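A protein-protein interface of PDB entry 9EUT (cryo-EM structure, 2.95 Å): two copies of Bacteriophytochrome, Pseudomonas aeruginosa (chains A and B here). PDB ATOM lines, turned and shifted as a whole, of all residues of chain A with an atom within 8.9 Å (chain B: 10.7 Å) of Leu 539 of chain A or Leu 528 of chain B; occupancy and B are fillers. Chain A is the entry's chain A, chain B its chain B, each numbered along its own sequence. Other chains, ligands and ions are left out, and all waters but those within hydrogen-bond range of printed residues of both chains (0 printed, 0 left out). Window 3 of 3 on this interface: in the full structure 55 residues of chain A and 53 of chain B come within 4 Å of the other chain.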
ATOM      1  N   ILE A 522      34.563  20.355 -14.155  1.00  0.00           N
ATOM      2  CA  ILE A 522      33.584  19.379 -13.678  1.00  0.00           C
ATOM      3  C   ILE A 522      32.824  19.908 -12.465  1.00  0.00           C
ATOM      4  O   ILE A 522      31.603  19.739 -12.365  1.00  0.00           O
ATOM      5  CB  ILE A 522      34.257  18.027 -13.387  1.00  0.00           C
ATOM      6  CG1 ILE A 522      34.793  17.424 -14.682  1.00  0.00           C
ATOM      7  CG2 ILE A 522      33.282  17.070 -12.717  1.00  0.00           C
ATOM      8  CD1 ILE A 522      35.725  16.276 -14.472  1.00  0.00           C
ATOM      9  N   ALA A 526      28.823  20.465 -12.337  1.00  0.00           N
ATOM     10  CA  ALA A 526      27.993  19.875 -11.292  1.00  0.00           C
ATOM     11  C   ALA A 526      27.192  20.944 -10.559  1.00  0.00           C
ATOM     12  O   ALA A 526      26.018  20.737 -10.234  1.00  0.00           O
ATOM     13  CB  ALA A 526      28.861  19.086 -10.312  1.00  0.00           C
ATOM     14  N   LEU A 529      24.165  21.914 -12.645  1.00  0.00           N
ATOM     15  CA  LEU A 529      23.065  20.968 -12.788  1.00  0.00           C
ATOM     16  C   LEU A 529      21.830  21.455 -12.039  1.00  0.00           C
ATOM     17  O   LEU A 529      21.894  21.786 -10.851  1.00  0.00           O
ATOM     18  CB  LEU A 529      23.484  19.592 -12.272  1.00  0.00           C
ATOM     19  CG  LEU A 529      24.423  18.781 -13.164  1.00  0.00           C
ATOM     20  CD1 LEU A 529      24.914  17.544 -12.432  1.00  0.00           C
ATOM     21  CD2 LEU A 529      23.725  18.399 -14.458  1.00  0.00           C
ATOM     22  N   SER A 531      19.391  19.919 -10.882  1.00  0.00           N
ATOM     23  CA  SER A 531      18.997  19.048  -9.773  1.00  0.00           C
ATOM     24  C   SER A 531      17.479  18.883  -9.691  1.00  0.00           C
ATOM     25  O   SER A 531      16.925  18.657  -8.612  1.00  0.00           O
ATOM     26  CB  SER A 531      19.550  19.575  -8.446  1.00  0.00           C
ATOM     27  OG  SER A 531      19.838  18.522  -7.550  1.00  0.00           O
ATOM     28  N   ASP A 533      15.515  16.452 -10.938  1.00  0.00           N
ATOM     29  CA  ASP A 533      15.178  15.085 -10.572  1.00  0.00           C
ATOM     30  C   ASP A 533      15.991  14.602  -9.378  1.00  0.00           C
ATOM     31  O   ASP A 533      17.139  15.006  -9.175  1.00  0.00           O
ATOM     32  CB  ASP A 533      15.402  14.142 -11.757  1.00  0.00           C
ATOM     33  CG  ASP A 533      14.128  13.859 -12.525  1.00  0.00           C
ATOM     34  OD1 ASP A 533      13.049  14.297 -12.074  1.00  0.00           O
ATOM     35  OD2 ASP A 533      14.205  13.198 -13.583  1.00  0.00           O
ATOM     36  N   THR A 534      15.368  13.729  -8.579  1.00  0.00           N
ATOM     37  CA  THR A 534      16.057  13.139  -7.434  1.00  0.00           C
ATOM     38  C   THR A 534      17.272  12.340  -7.884  1.00  0.00           C
ATOM     39  O   THR A 534      18.317  12.358  -7.223  1.00  0.00           O
ATOM     40  CB  THR A 534      15.098  12.253  -6.639  1.00  0.00           C
ATOM     41  OG1 THR A 534      14.218  11.571  -7.540  1.00  0.00           O
ATOM     42  CG2 THR A 534      14.277  13.094  -5.673  1.00  0.00           C
ATOM     43  N   ARG A 535      17.150  11.622  -9.003  1.00  0.00           N
ATOM     44  CA  ARG A 535      18.297  10.900  -9.543  1.00  0.00           C
ATOM     45  C   ARG A 535      19.386  11.883  -9.948  1.00  0.00           C
ATOM     46  O   ARG A 535      20.571  11.682  -9.650  1.00  0.00           O
ATOM     47  CB  ARG A 535      17.865  10.046 -10.734  1.00  0.00           C
ATOM     48  CG  ARG A 535      18.807   8.902 -11.061  1.00  0.00           C
ATOM     49  CD  ARG A 535      18.313   8.115 -12.264  1.00  0.00           C
ATOM     50  NE  ARG A 535      19.081   6.893 -12.470  1.00  0.00           N
ATOM     51  CZ  ARG A 535      18.917   6.070 -13.496  1.00  0.00           C
ATOM     52  NH1 ARG A 535      18.074   6.347 -14.477  1.00  0.00           N
ATOM     53  NH2 ARG A 535      19.636   4.952 -13.552  1.00  0.00           N
ATOM     54  N   THR A 536      18.991  12.959 -10.633  1.00  0.00           N
ATOM     55  CA  THR A 536      19.940  13.995 -11.021  1.00  0.00           C
ATOM     56  C   THR A 536      20.554  14.648  -9.791  1.00  0.00           C
ATOM     57  O   THR A 536      21.737  14.994  -9.789  1.00  0.00           O
ATOM     58  CB  THR A 536      19.250  15.042 -11.896  1.00  0.00           C
ATOM     59  OG1 THR A 536      18.470  14.386 -12.904  1.00  0.00           O
ATOM     60  CG2 THR A 536      20.278  15.941 -12.564  1.00  0.00           C
ATOM     61  N   THR A 537      19.765  14.803  -8.726  1.00  0.00           N
ATOM     62  CA  THR A 537      20.270  15.381  -7.484  1.00  0.00           C
ATOM     63  C   THR A 537      21.331  14.491  -6.848  1.00  0.00           C
ATOM     64  O   THR A 537      22.401  14.968  -6.450  1.00  0.00           O
ATOM     65  CB  THR A 537      19.115  15.612  -6.509  1.00  0.00           C
ATOM     66  OG1 THR A 537      18.119  16.435  -7.130  1.00  0.00           O
ATOM     67  CG2 THR A 537      19.613  16.289  -5.240  1.00  0.00           C
ATOM     68  N   GLU A 538      21.049  13.192  -6.744  1.00  0.00           N
ATOM     69  CA  GLU A 538      22.015  12.257  -6.176  1.00  0.00           C
ATOM     70  C   GLU A 538      23.287  12.197  -7.014  1.00  0.00           C
ATOM     71  O   GLU A 538      24.400  12.197  -6.469  1.00  0.00           O
ATOM     72  CB  GLU A 538      21.384  10.870  -6.059  1.00  0.00           C
ATOM     73  CG  GLU A 538      20.366  10.747  -4.939  1.00  0.00           C
ATOM     74  CD  GLU A 538      19.670   9.400  -4.930  1.00  0.00           C
ATOM     75  OE1 GLU A 538      20.052   8.527  -5.738  1.00  0.00           O
ATOM     76  OE2 GLU A 538      18.742   9.213  -4.115  1.00  0.00           O
ATOM     77  N   LEU A 539      23.147  12.160  -8.341  1.00  0.00           N
ATOM     78  CA  LEU A 539      24.326  12.136  -9.201  1.00  0.00           C
ATOM     79  C   LEU A 539      25.127  13.425  -9.069  1.00  0.00           C
ATOM     80  O   LEU A 539      26.360  13.388  -9.006  1.00  0.00           O
ATOM     81  CB  LEU A 539      23.912  11.901 -10.654  1.00  0.00           C
ATOM     82  CG  LEU A 539      23.295  10.534 -10.962  1.00  0.00           C
ATOM     83  CD1 LEU A 539      22.670  10.522 -12.350  1.00  0.00           C
ATOM     84  CD2 LEU A 539      24.333   9.431 -10.830  1.00  0.00           C
ATOM     85  N   ARG A 540      24.447  14.573  -9.051  1.00  0.00           N
ATOM     86  CA  ARG A 540      25.115  15.856  -8.871  1.00  0.00           C
ATOM     87  C   ARG A 540      25.888  15.900  -7.562  1.00  0.00           C
ATOM     88  O   ARG A 540      27.032  16.369  -7.520  1.00  0.00           O
ATOM     89  CB  ARG A 540      24.083  16.980  -8.916  1.00  0.00           C
ATOM     90  CG  ARG A 540      24.655  18.362  -8.699  1.00  0.00           C
ATOM     91  CD  ARG A 540      23.554  19.403  -8.733  1.00  0.00           C
ATOM     92  NE  ARG A 540      22.713  19.340  -7.545  1.00  0.00           N
ATOM     93  CZ  ARG A 540      22.948  20.007  -6.425  1.00  0.00           C
ATOM     94  NH1 ARG A 540      24.067  20.692  -6.250  1.00  0.00           N
ATOM     95  NH2 ARG A 540      22.058  19.951  -5.438  1.00  0.00           N
ATOM     96  N   GLN A 541      25.275  15.417  -6.479  1.00  0.00           N
ATOM     97  CA  GLN A 541      25.950  15.390  -5.186  1.00  0.00           C
ATOM     98  C   GLN A 541      27.174  14.482  -5.210  1.00  0.00           C
ATOM     99  O   GLN A 541      28.239  14.852  -4.701  1.00  0.00           O
ATOM    100  CB  GLN A 541      24.968  14.934  -4.110  1.00  0.00           C
ATOM    101  CG  GLN A 541      23.943  15.987  -3.727  1.00  0.00           C
ATOM    102  CD  GLN A 541      22.832  15.427  -2.861  1.00  0.00           C
ATOM    103  OE1 GLN A 541      22.700  14.212  -2.710  1.00  0.00           O
ATOM    104  NE2 GLN A 541      22.022  16.312  -2.292  1.00  0.00           N
ATOM    105  N   HIS A 542      27.047  13.294  -5.807  1.00  0.00           N
ATOM    106  CA  HIS A 542      28.184  12.380  -5.877  1.00  0.00           C
ATOM    107  C   HIS A 542      29.314  12.957  -6.722  1.00  0.00           C
ATOM    108  O   HIS A 542      30.494  12.835  -6.367  1.00  0.00           O
ATOM    109  CB  HIS A 542      27.736  11.028  -6.429  1.00  0.00           C
ATOM    110  CG  HIS A 542      28.310   9.858  -5.693  1.00  0.00           C
ATOM    111  ND1 HIS A 542      29.645   9.522  -5.755  1.00  0.00           N
ATOM    112  CD2 HIS A 542      27.730   8.949  -4.875  1.00  0.00           C
ATOM    113  CE1 HIS A 542      29.862   8.454  -5.008  1.00  0.00           C
ATOM    114  NE2 HIS A 542      28.716   8.086  -4.463  1.00  0.00           N
ATOM    115  N   ILE A 543      28.969  13.629  -7.822  1.00  0.00           N
ATOM    116  CA  ILE A 543      29.971  14.254  -8.679  1.00  0.00           C
ATOM    117  C   ILE A 543      30.667  15.394  -7.953  1.00  0.00           C
ATOM    118  O   ILE A 543      31.895  15.523  -8.012  1.00  0.00           O
ATOM    119  CB  ILE A 543      29.324  14.731  -9.992  1.00  0.00           C
ATOM    120  CG1 ILE A 543      28.898  13.532 -10.839  1.00  0.00           C
ATOM    121  CG2 ILE A 543      30.275  15.633 -10.764  1.00  0.00           C
ATOM    122  CD1 ILE A 543      27.919  13.879 -11.936  1.00  0.00           C
ATOM    123  N   SER A 544      29.906  16.235  -7.254  1.00  0.00           N
ATOM    124  CA  SER A 544      30.512  17.337  -6.516  1.00  0.00           C
ATOM    125  C   SER A 544      31.426  16.822  -5.411  1.00  0.00           C
ATOM    126  O   SER A 544      32.527  17.350  -5.211  1.00  0.00           O
ATOM    127  CB  SER A 544      29.422  18.241  -5.940  1.00  0.00           C
ATOM    128  OG  SER A 544      29.982  19.400  -5.351  1.00  0.00           O
ATOM    129  N   ALA A 545      31.002  15.773  -4.705  1.00  0.00           N
ATOM    130  CA  ALA A 545      31.831  15.197  -3.650  1.00  0.00           C
ATOM    131  C   ALA A 545      33.125  14.612  -4.208  1.00  0.00           C
ATOM    132  O   ALA A 545      34.214  14.866  -3.677  1.00  0.00           O
ATOM    133  CB  ALA A 545      31.040  14.128  -2.894  1.00  0.00           C
ATOM    134  N   SER A 546      33.028  13.819  -5.278  1.00  0.00           N
ATOM    135  CA  SER A 546      34.228  13.235  -5.872  1.00  0.00           C
ATOM    136  C   SER A 546      35.157  14.309  -6.431  1.00  0.00           C
ATOM    137  O   SER A 546      36.385  14.206  -6.303  1.00  0.00           O
ATOM    138  CB  SER A 546      33.838  12.239  -6.962  1.00  0.00           C
ATOM    139  OG  SER A 546      33.067  11.176  -6.426  1.00  0.00           O
ATOM    140  N   SER A 547      34.595  15.358  -7.037  1.00  0.00           N
ATOM    141  CA  SER A 547      35.427  16.436  -7.556  1.00  0.00           C
ATOM    142  C   SER A 547      36.133  17.174  -6.428  1.00  0.00           C
ATOM    143  O   SER A 547      37.311  17.528  -6.555  1.00  0.00           O
ATOM    144  CB  SER A 547      34.577  17.401  -8.381  1.00  0.00           C
ATOM    145  OG  SER A 547      33.997  16.745  -9.495  1.00  0.00           O
ATOM    146  N   PRO B 518      38.055   8.118  -7.709  1.00  0.00           N
ATOM    147  CA  PRO B 518      37.128   9.247  -7.925  1.00  0.00           C
ATOM    148  C   PRO B 518      36.846   9.529  -9.390  1.00  0.00           C
ATOM    149  O   PRO B 518      35.708   9.871  -9.747  1.00  0.00           O
ATOM    150  CB  PRO B 518      37.834  10.436  -7.255  1.00  0.00           C
ATOM    151  CG  PRO B 518      39.214  10.004  -6.977  1.00  0.00           C
ATOM    152  CD  PRO B 518      39.258   8.519  -6.959  1.00  0.00           C
ATOM    153  N   GLN B 520      36.824   7.273 -11.851  1.00  0.00           N
ATOM    154  CA  GLN B 520      35.899   6.231 -12.286  1.00  0.00           C
ATOM    155  C   GLN B 520      34.487   6.513 -11.783  1.00  0.00           C
ATOM    156  O   GLN B 520      33.508   6.316 -12.513  1.00  0.00           O
ATOM    157  CB  GLN B 520      36.380   4.867 -11.794  1.00  0.00           C
ATOM    158  CG  GLN B 520      36.692   3.879 -12.903  1.00  0.00           C
ATOM    159  CD  GLN B 520      37.246   2.571 -12.372  1.00  0.00           C
ATOM    160  OE1 GLN B 520      37.413   2.400 -11.165  1.00  0.00           O
ATOM    161  NE2 GLN B 520      37.535   1.642 -13.275  1.00  0.00           N
ATOM    162  N   SER B 521      34.368   6.978 -10.537  1.00  0.00           N
ATOM    163  CA  SER B 521      33.062   7.311  -9.974  1.00  0.00           C
ATOM    164  C   SER B 521      32.376   8.417 -10.768  1.00  0.00           C
ATOM    165  O   SER B 521      31.182   8.325 -11.083  1.00  0.00           O
ATOM    166  CB  SER B 521      33.216   7.714  -8.507  1.00  0.00           C
ATOM    167  OG  SER B 521      31.953   7.903  -7.895  1.00  0.00           O
ATOM    168  N   ILE B 522      33.119   9.472 -11.112  1.00  0.00           N
ATOM    169  CA  ILE B 522      32.538  10.559 -11.899  1.00  0.00           C
ATOM    170  C   ILE B 522      32.158  10.085 -13.298  1.00  0.00           C
ATOM    171  O   ILE B 522      31.099  10.451 -13.817  1.00  0.00           O
ATOM    172  CB  ILE B 522      33.473  11.780 -11.938  1.00  0.00           C
ATOM    173  CG1 ILE B 522      33.611  12.368 -10.536  1.00  0.00           C
ATOM    174  CG2 ILE B 522      32.952  12.833 -12.902  1.00  0.00           C
ATOM    175  CD1 ILE B 522      34.734  13.341 -10.394  1.00  0.00           C
ATOM    176  N   SER B 523      33.025   9.309 -13.948  1.00  0.00           N
ATOM    177  CA  SER B 523      32.698   8.797 -15.278  1.00  0.00           C
ATOM    178  C   SER B 523      31.438   7.935 -15.249  1.00  0.00           C
ATOM    179  O   SER B 523      30.580   8.045 -16.136  1.00  0.00           O
ATOM    180  CB  SER B 523      33.879   8.006 -15.838  1.00  0.00           C
ATOM    181  OG  SER B 523      34.865   8.872 -16.370  1.00  0.00           O
ATOM    182  N   MET B 524      31.285   7.109 -14.213  1.00  0.00           N
ATOM    183  CA  MET B 524      30.083   6.291 -14.079  1.00  0.00           C
ATOM    184  C   MET B 524      28.848   7.156 -13.850  1.00  0.00           C
ATOM    185  O   MET B 524      27.802   6.942 -14.477  1.00  0.00           O
ATOM    186  CB  MET B 524      30.258   5.292 -12.935  1.00  0.00           C
ATOM    187  CG  MET B 524      30.534   3.871 -13.388  1.00  0.00           C
ATOM    188  SD  MET B 524      32.177   3.694 -14.109  1.00  0.00           S
ATOM    189  CE  MET B 524      33.063   2.945 -12.746  1.00  0.00           C
ATOM    190  N   ALA B 525      28.954   8.145 -12.960  1.00  0.00           N
ATOM    191  CA  ALA B 525      27.817   9.025 -12.706  1.00  0.00           C
ATOM    192  C   ALA B 525      27.425   9.786 -13.966  1.00  0.00           C
ATOM    193  O   ALA B 525      26.233   9.977 -14.239  1.00  0.00           O
ATOM    194  CB  ALA B 525      28.146   9.992 -11.571  1.00  0.00           C
ATOM    195  N   ALA B 526      28.412  10.233 -14.744  1.00  0.00           N
ATOM    196  CA  ALA B 526      28.115  10.910 -16.000  1.00  0.00           C
ATOM    197  C   ALA B 526      27.409   9.969 -16.965  1.00  0.00           C
ATOM    198  O   ALA B 526      26.422  10.347 -17.603  1.00  0.00           O
ATOM    199  CB  ALA B 526      29.400  11.457 -16.621  1.00  0.00           C
ATOM    200  N   ALA B 527      27.882   8.723 -17.062  1.00  0.00           N
ATOM    201  CA  ALA B 527      27.226   7.747 -17.925  1.00  0.00           C
ATOM    202  C   ALA B 527      25.798   7.470 -17.473  1.00  0.00           C
ATOM    203  O   ALA B 527      24.950   7.087 -18.288  1.00  0.00           O
ATOM    204  CB  ALA B 527      28.033   6.450 -17.963  1.00  0.00           C
ATOM    205  N   LEU B 528      25.512   7.659 -16.185  1.00  0.00           N
ATOM    206  CA  LEU B 528      24.174   7.451 -15.643  1.00  0.00           C
ATOM    207  C   LEU B 528      23.246   8.649 -15.820  1.00  0.00           C
ATOM    208  O   LEU B 528      22.036   8.500 -15.614  1.00  0.00           O
ATOM    209  CB  LEU B 528      24.258   7.090 -14.159  1.00  0.00           C
ATOM    210  CG  LEU B 528      24.835   5.710 -13.838  1.00  0.00           C
ATOM    211  CD1 LEU B 528      25.148   5.590 -12.357  1.00  0.00           C
ATOM    212  CD2 LEU B 528      23.878   4.614 -14.278  1.00  0.00           C
ATOM    213  N   LEU B 529      23.766   9.821 -16.182  1.00  0.00           N
ATOM    214  CA  LEU B 529      22.920  10.995 -16.378  1.00  0.00           C
ATOM    215  C   LEU B 529      21.930  10.787 -17.521  1.00  0.00           C
ATOM    216  O   LEU B 529      22.324  10.582 -18.673  1.00  0.00           O
ATOM    217  CB  LEU B 529      23.790  12.220 -16.650  1.00  0.00           C
ATOM    218  CG  LEU B 529      24.471  12.850 -15.435  1.00  0.00           C
ATOM    219  CD1 LEU B 529      25.488  13.888 -15.875  1.00  0.00           C
ATOM    220  CD2 LEU B 529      23.436  13.468 -14.509  1.00  0.00           C
ATOM    221  N   SER B 530      20.638  10.839 -17.180  1.00  0.00           N
ATOM    222  CA  SER B 530      19.552  10.596 -18.128  1.00  0.00           C
ATOM    223  C   SER B 530      19.586  11.512 -19.348  1.00  0.00           C
ATOM    224  O   SER B 530      19.051  11.136 -20.396  1.00  0.00           O
ATOM    225  CB  SER B 530      18.204  10.738 -17.419  1.00  0.00           C
ATOM    226  OG  SER B 530      17.979  12.077 -17.015  1.00  0.00           O
ATOM    227  N   SER B 531      20.199  12.695 -19.241  1.00  0.00           N
ATOM    228  CA  SER B 531      20.313  13.633 -20.362  1.00  0.00           C
ATOM    229  C   SER B 531      18.945  13.986 -20.947  1.00  0.00           C
ATOM    230  O   SER B 531      18.786  14.124 -22.162  1.00  0.00           O
ATOM    231  CB  SER B 531      21.234  13.085 -21.453  1.00  0.00           C
ATOM    232  OG  SER B 531      22.483  12.705 -20.914  1.00  0.00           O
ATOM    233  N   SER B 532      17.948  14.128 -20.072  1.00  0.00           N
ATOM    234  CA  SER B 532      16.604  14.484 -20.522  1.00  0.00           C
ATOM    235  C   SER B 532      16.580  15.866 -21.166  1.00  0.00           C
ATOM    236  O   SER B 532      15.967  16.056 -22.223  1.00  0.00           O
ATOM    237  CB  SER B 532      15.626  14.424 -19.350  1.00  0.00           C
ATOM    238  OG  SER B 532      16.082  15.217 -18.266  1.00  0.00           O
ATOM    239  N   THR B 536      21.298  19.443 -19.767  1.00  0.00           N
ATOM    240  CA  THR B 536      21.807  18.306 -19.006  1.00  0.00           C
ATOM    241  C   THR B 536      22.670  17.405 -19.881  1.00  0.00           C
ATOM    242  O   THR B 536      23.695  16.882 -19.431  1.00  0.00           O
ATOM    243  CB  THR B 536      20.646  17.513 -18.405  1.00  0.00           C
ATOM    244  OG1 THR B 536      19.730  18.410 -17.767  1.00  0.00           O
ATOM    245  CG2 THR B 536      21.156  16.506 -17.385  1.00  0.00           C
ATOM    246  N   THR B 537      22.287  17.245 -21.149  1.00  0.00           N
ATOM    247  CA  THR B 537      23.064  16.437 -22.084  1.00  0.00           C
ATOM    248  C   THR B 537      24.428  17.064 -22.352  1.00  0.00           C
ATOM    249  O   THR B 537      25.455  16.374 -22.344  1.00  0.00           O
ATOM    250  CB  THR B 537      22.291  16.258 -23.390  1.00  0.00           C
ATOM    251  OG1 THR B 537      20.958  15.818 -23.100  1.00  0.00           O
ATOM    252  CG2 THR B 537      22.976  15.229 -24.273  1.00  0.00           C
ATOM    253  N   LEU B 539      26.026  19.205 -20.401  1.00  0.00           N
ATOM    254  CA  LEU B 539      26.813  19.114 -19.175  1.00  0.00           C
ATOM    255  C   LEU B 539      27.380  17.710 -18.995  1.00  0.00           C
ATOM    256  O   LEU B 539      28.542  17.549 -18.604  1.00  0.00           O
ATOM    257  CB  LEU B 539      25.960  19.512 -17.972  1.00  0.00           C
ATOM    258  CG  LEU B 539      25.575  20.991 -17.876  1.00  0.00           C
ATOM    259  CD1 LEU B 539      24.501  21.202 -16.820  1.00  0.00           C
ATOM    260  CD2 LEU B 539      26.796  21.848 -17.582  1.00  0.00           C
ATOM    261  N   ARG B 540      26.567  16.683 -19.255  1.00  0.00           N
ATOM    262  CA  ARG B 540      27.046  15.307 -19.179  1.00  0.00           C
ATOM    263  C   ARG B 540      28.208  15.081 -20.134  1.00  0.00           C
ATOM    264  O   ARG B 540      29.208  14.447 -19.780  1.00  0.00           O
ATOM    265  CB  ARG B 540      25.909  14.336 -19.488  1.00  0.00           C
ATOM    266  CG  ARG B 540      26.336  12.886 -19.425  1.00  0.00           C
ATOM    267  CD  ARG B 540      25.234  11.965 -19.896  1.00  0.00           C
ATOM    268  NE  ARG B 540      24.939  12.146 -21.310  1.00  0.00           N
ATOM    269  CZ  ARG B 540      25.508  11.455 -22.288  1.00  0.00           C
ATOM    270  NH1 ARG B 540      26.517  10.632 -22.054  1.00  0.00           N
ATOM    271  NH2 ARG B 540      25.086  11.629 -23.537  1.00  0.00           N
ATOM    272  N   GLN B 541      28.076  15.573 -21.367  1.00  0.00           N
ATOM    273  CA  GLN B 541      29.141  15.428 -22.353  1.00  0.00           C
ATOM    274  C   GLN B 541      30.420  16.117 -21.895  1.00  0.00           C
ATOM    275  O   GLN B 541      31.517  15.562 -22.029  1.00  0.00           O
ATOM    276  CB  GLN B 541      28.682  15.994 -23.696  1.00  0.00           C
ATOM    277  CG  GLN B 541      27.696  15.111 -24.439  1.00  0.00           C
ATOM    278  CD  GLN B 541      27.095  15.805 -25.646  1.00  0.00           C
ATOM    279  OE1 GLN B 541      27.368  16.978 -25.901  1.00  0.00           O
ATOM    280  NE2 GLN B 541      26.269  15.084 -26.393  1.00  0.00           N
ATOM    281  N   ILE B 543      31.334  16.791 -18.792  1.00  0.00           N
ATOM    282  CA  ILE B 543      31.874  16.038 -17.663  1.00  0.00           C
ATOM    283  C   ILE B 543      32.581  14.777 -18.142  1.00  0.00           C
ATOM    284  O   ILE B 543      33.680  14.453 -17.676  1.00  0.00           O
ATOM    285  CB  ILE B 543      30.752  15.715 -16.659  1.00  0.00           C
ATOM    286  CG1 ILE B 543      30.285  16.992 -15.959  1.00  0.00           C
ATOM    287  CG2 ILE B 543      31.215  14.677 -15.647  1.00  0.00           C
ATOM    288  CD1 ILE B 543      28.971  16.843 -15.229  1.00  0.00           C
ATOM    289  N   SER B 544      31.978  14.057 -19.085  1.00  0.00           N
ATOM    290  CA  SER B 544      32.596  12.840 -19.602  1.00  0.00           C
ATOM    291  C   SER B 544      33.898  13.149 -20.336  1.00  0.00           C
ATOM    292  O   SER B 544      34.890  12.429 -20.176  1.00  0.00           O
ATOM    293  CB  SER B 544      31.621  12.105 -20.519  1.00  0.00           C
ATOM    294  OG  SER B 544      32.138  10.841 -20.898  1.00  0.00           O
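The backbone carbonyl oxygen of His 542 of chain A lies within hydrogen-bond range of the side-chain hydroxyl of Ser 546 of chain A, 3.1 Å away. O of Leu 529 of chain B is in hydrogen-bond range of OG of Ser 531 of chain B. The backbone carbonyl oxygen (O) of Ile 543 of chain A is in hydrogen-bond range of the side-chain hydroxyl (OG) of Ser 547 of chain A.
Among the printed residues, merely in contact across the chains: His 542 of chain A with Ser 521 of chain B (3.5 Å), Ser 546 of chain A with Ile 522 of chain B (3.6 Å), Ser 547 of chain A with Ile 522 of chain B (3.6 Å), Ile 543 of chain A with Ala 525 of chain B (3.7 Å), Leu 539 of chain A with Leu 529 of chain B (3.7 Å), Leu 529 of chain A with Leu 539 of chain B (3.7 Å), Ser 546 of chain A with Ser 521 of chain B (3.8 Å), Leu 539 of chain A with Leu 528 of chain B (3.9 Å) and Leu 539 of chain A with Ala 525 of chain B (3.9 Å).
Leu 529 of chain A touches Leu 539 of chain B, and with the chains exchanged Leu 539 of chain A touches Leu 529 of chain B. Positions printed for both chains: 522, 526, 529, 531, 536, 537, 539, 540, 541, 543 and 544.
Leu 528 of chain B touches just one residue of chain A: Leu 539 (3.9 Å). Of chain B, only Ala 525 (3.7 Å) comes within 4 Å of Ile 543 of chain A. Ala 525 of chain B touches two residues of chain A. No residue of chain A comes within 4 Å of Ala 527 of chain B. Printed residues of chain A within 4 Å of Leu 539 of chain B: Leu 529. Of the printed residues of chain B, Ser 546 of chain A touches Ser 521 (3.8 Å) and Ile 522 (3.6 Å). Of the printed residues of chain A, Ser 521 of chain B touches His 542 and Ser 546. Of the printed residues of chain A, Ile 522 of chain B touches Ser 546 and Ser 547. Of the printed residues of chain B, Leu 529 of chain A touches Leu 539. Gln 541 of chain A touches none of the printed residues of chain B. Arg 540 of chain B touches none of the printed residues of chain A.
Of the 21 printed residues of chain B, 6 touch a printed residue of chain A. Printed residues of chain B that touch a printed residue of chain A: Ser 521, Ile 522, Ala 525, Leu 528, Leu 529 and Leu 539. Along chain A the printed residues that touch a printed residue of chain B span positions 529 to 547. Among the printed residues, no Asp or Glu carboxylate lies within 4 Å of a Lys or Arg side-chain nitrogen of the other chain.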
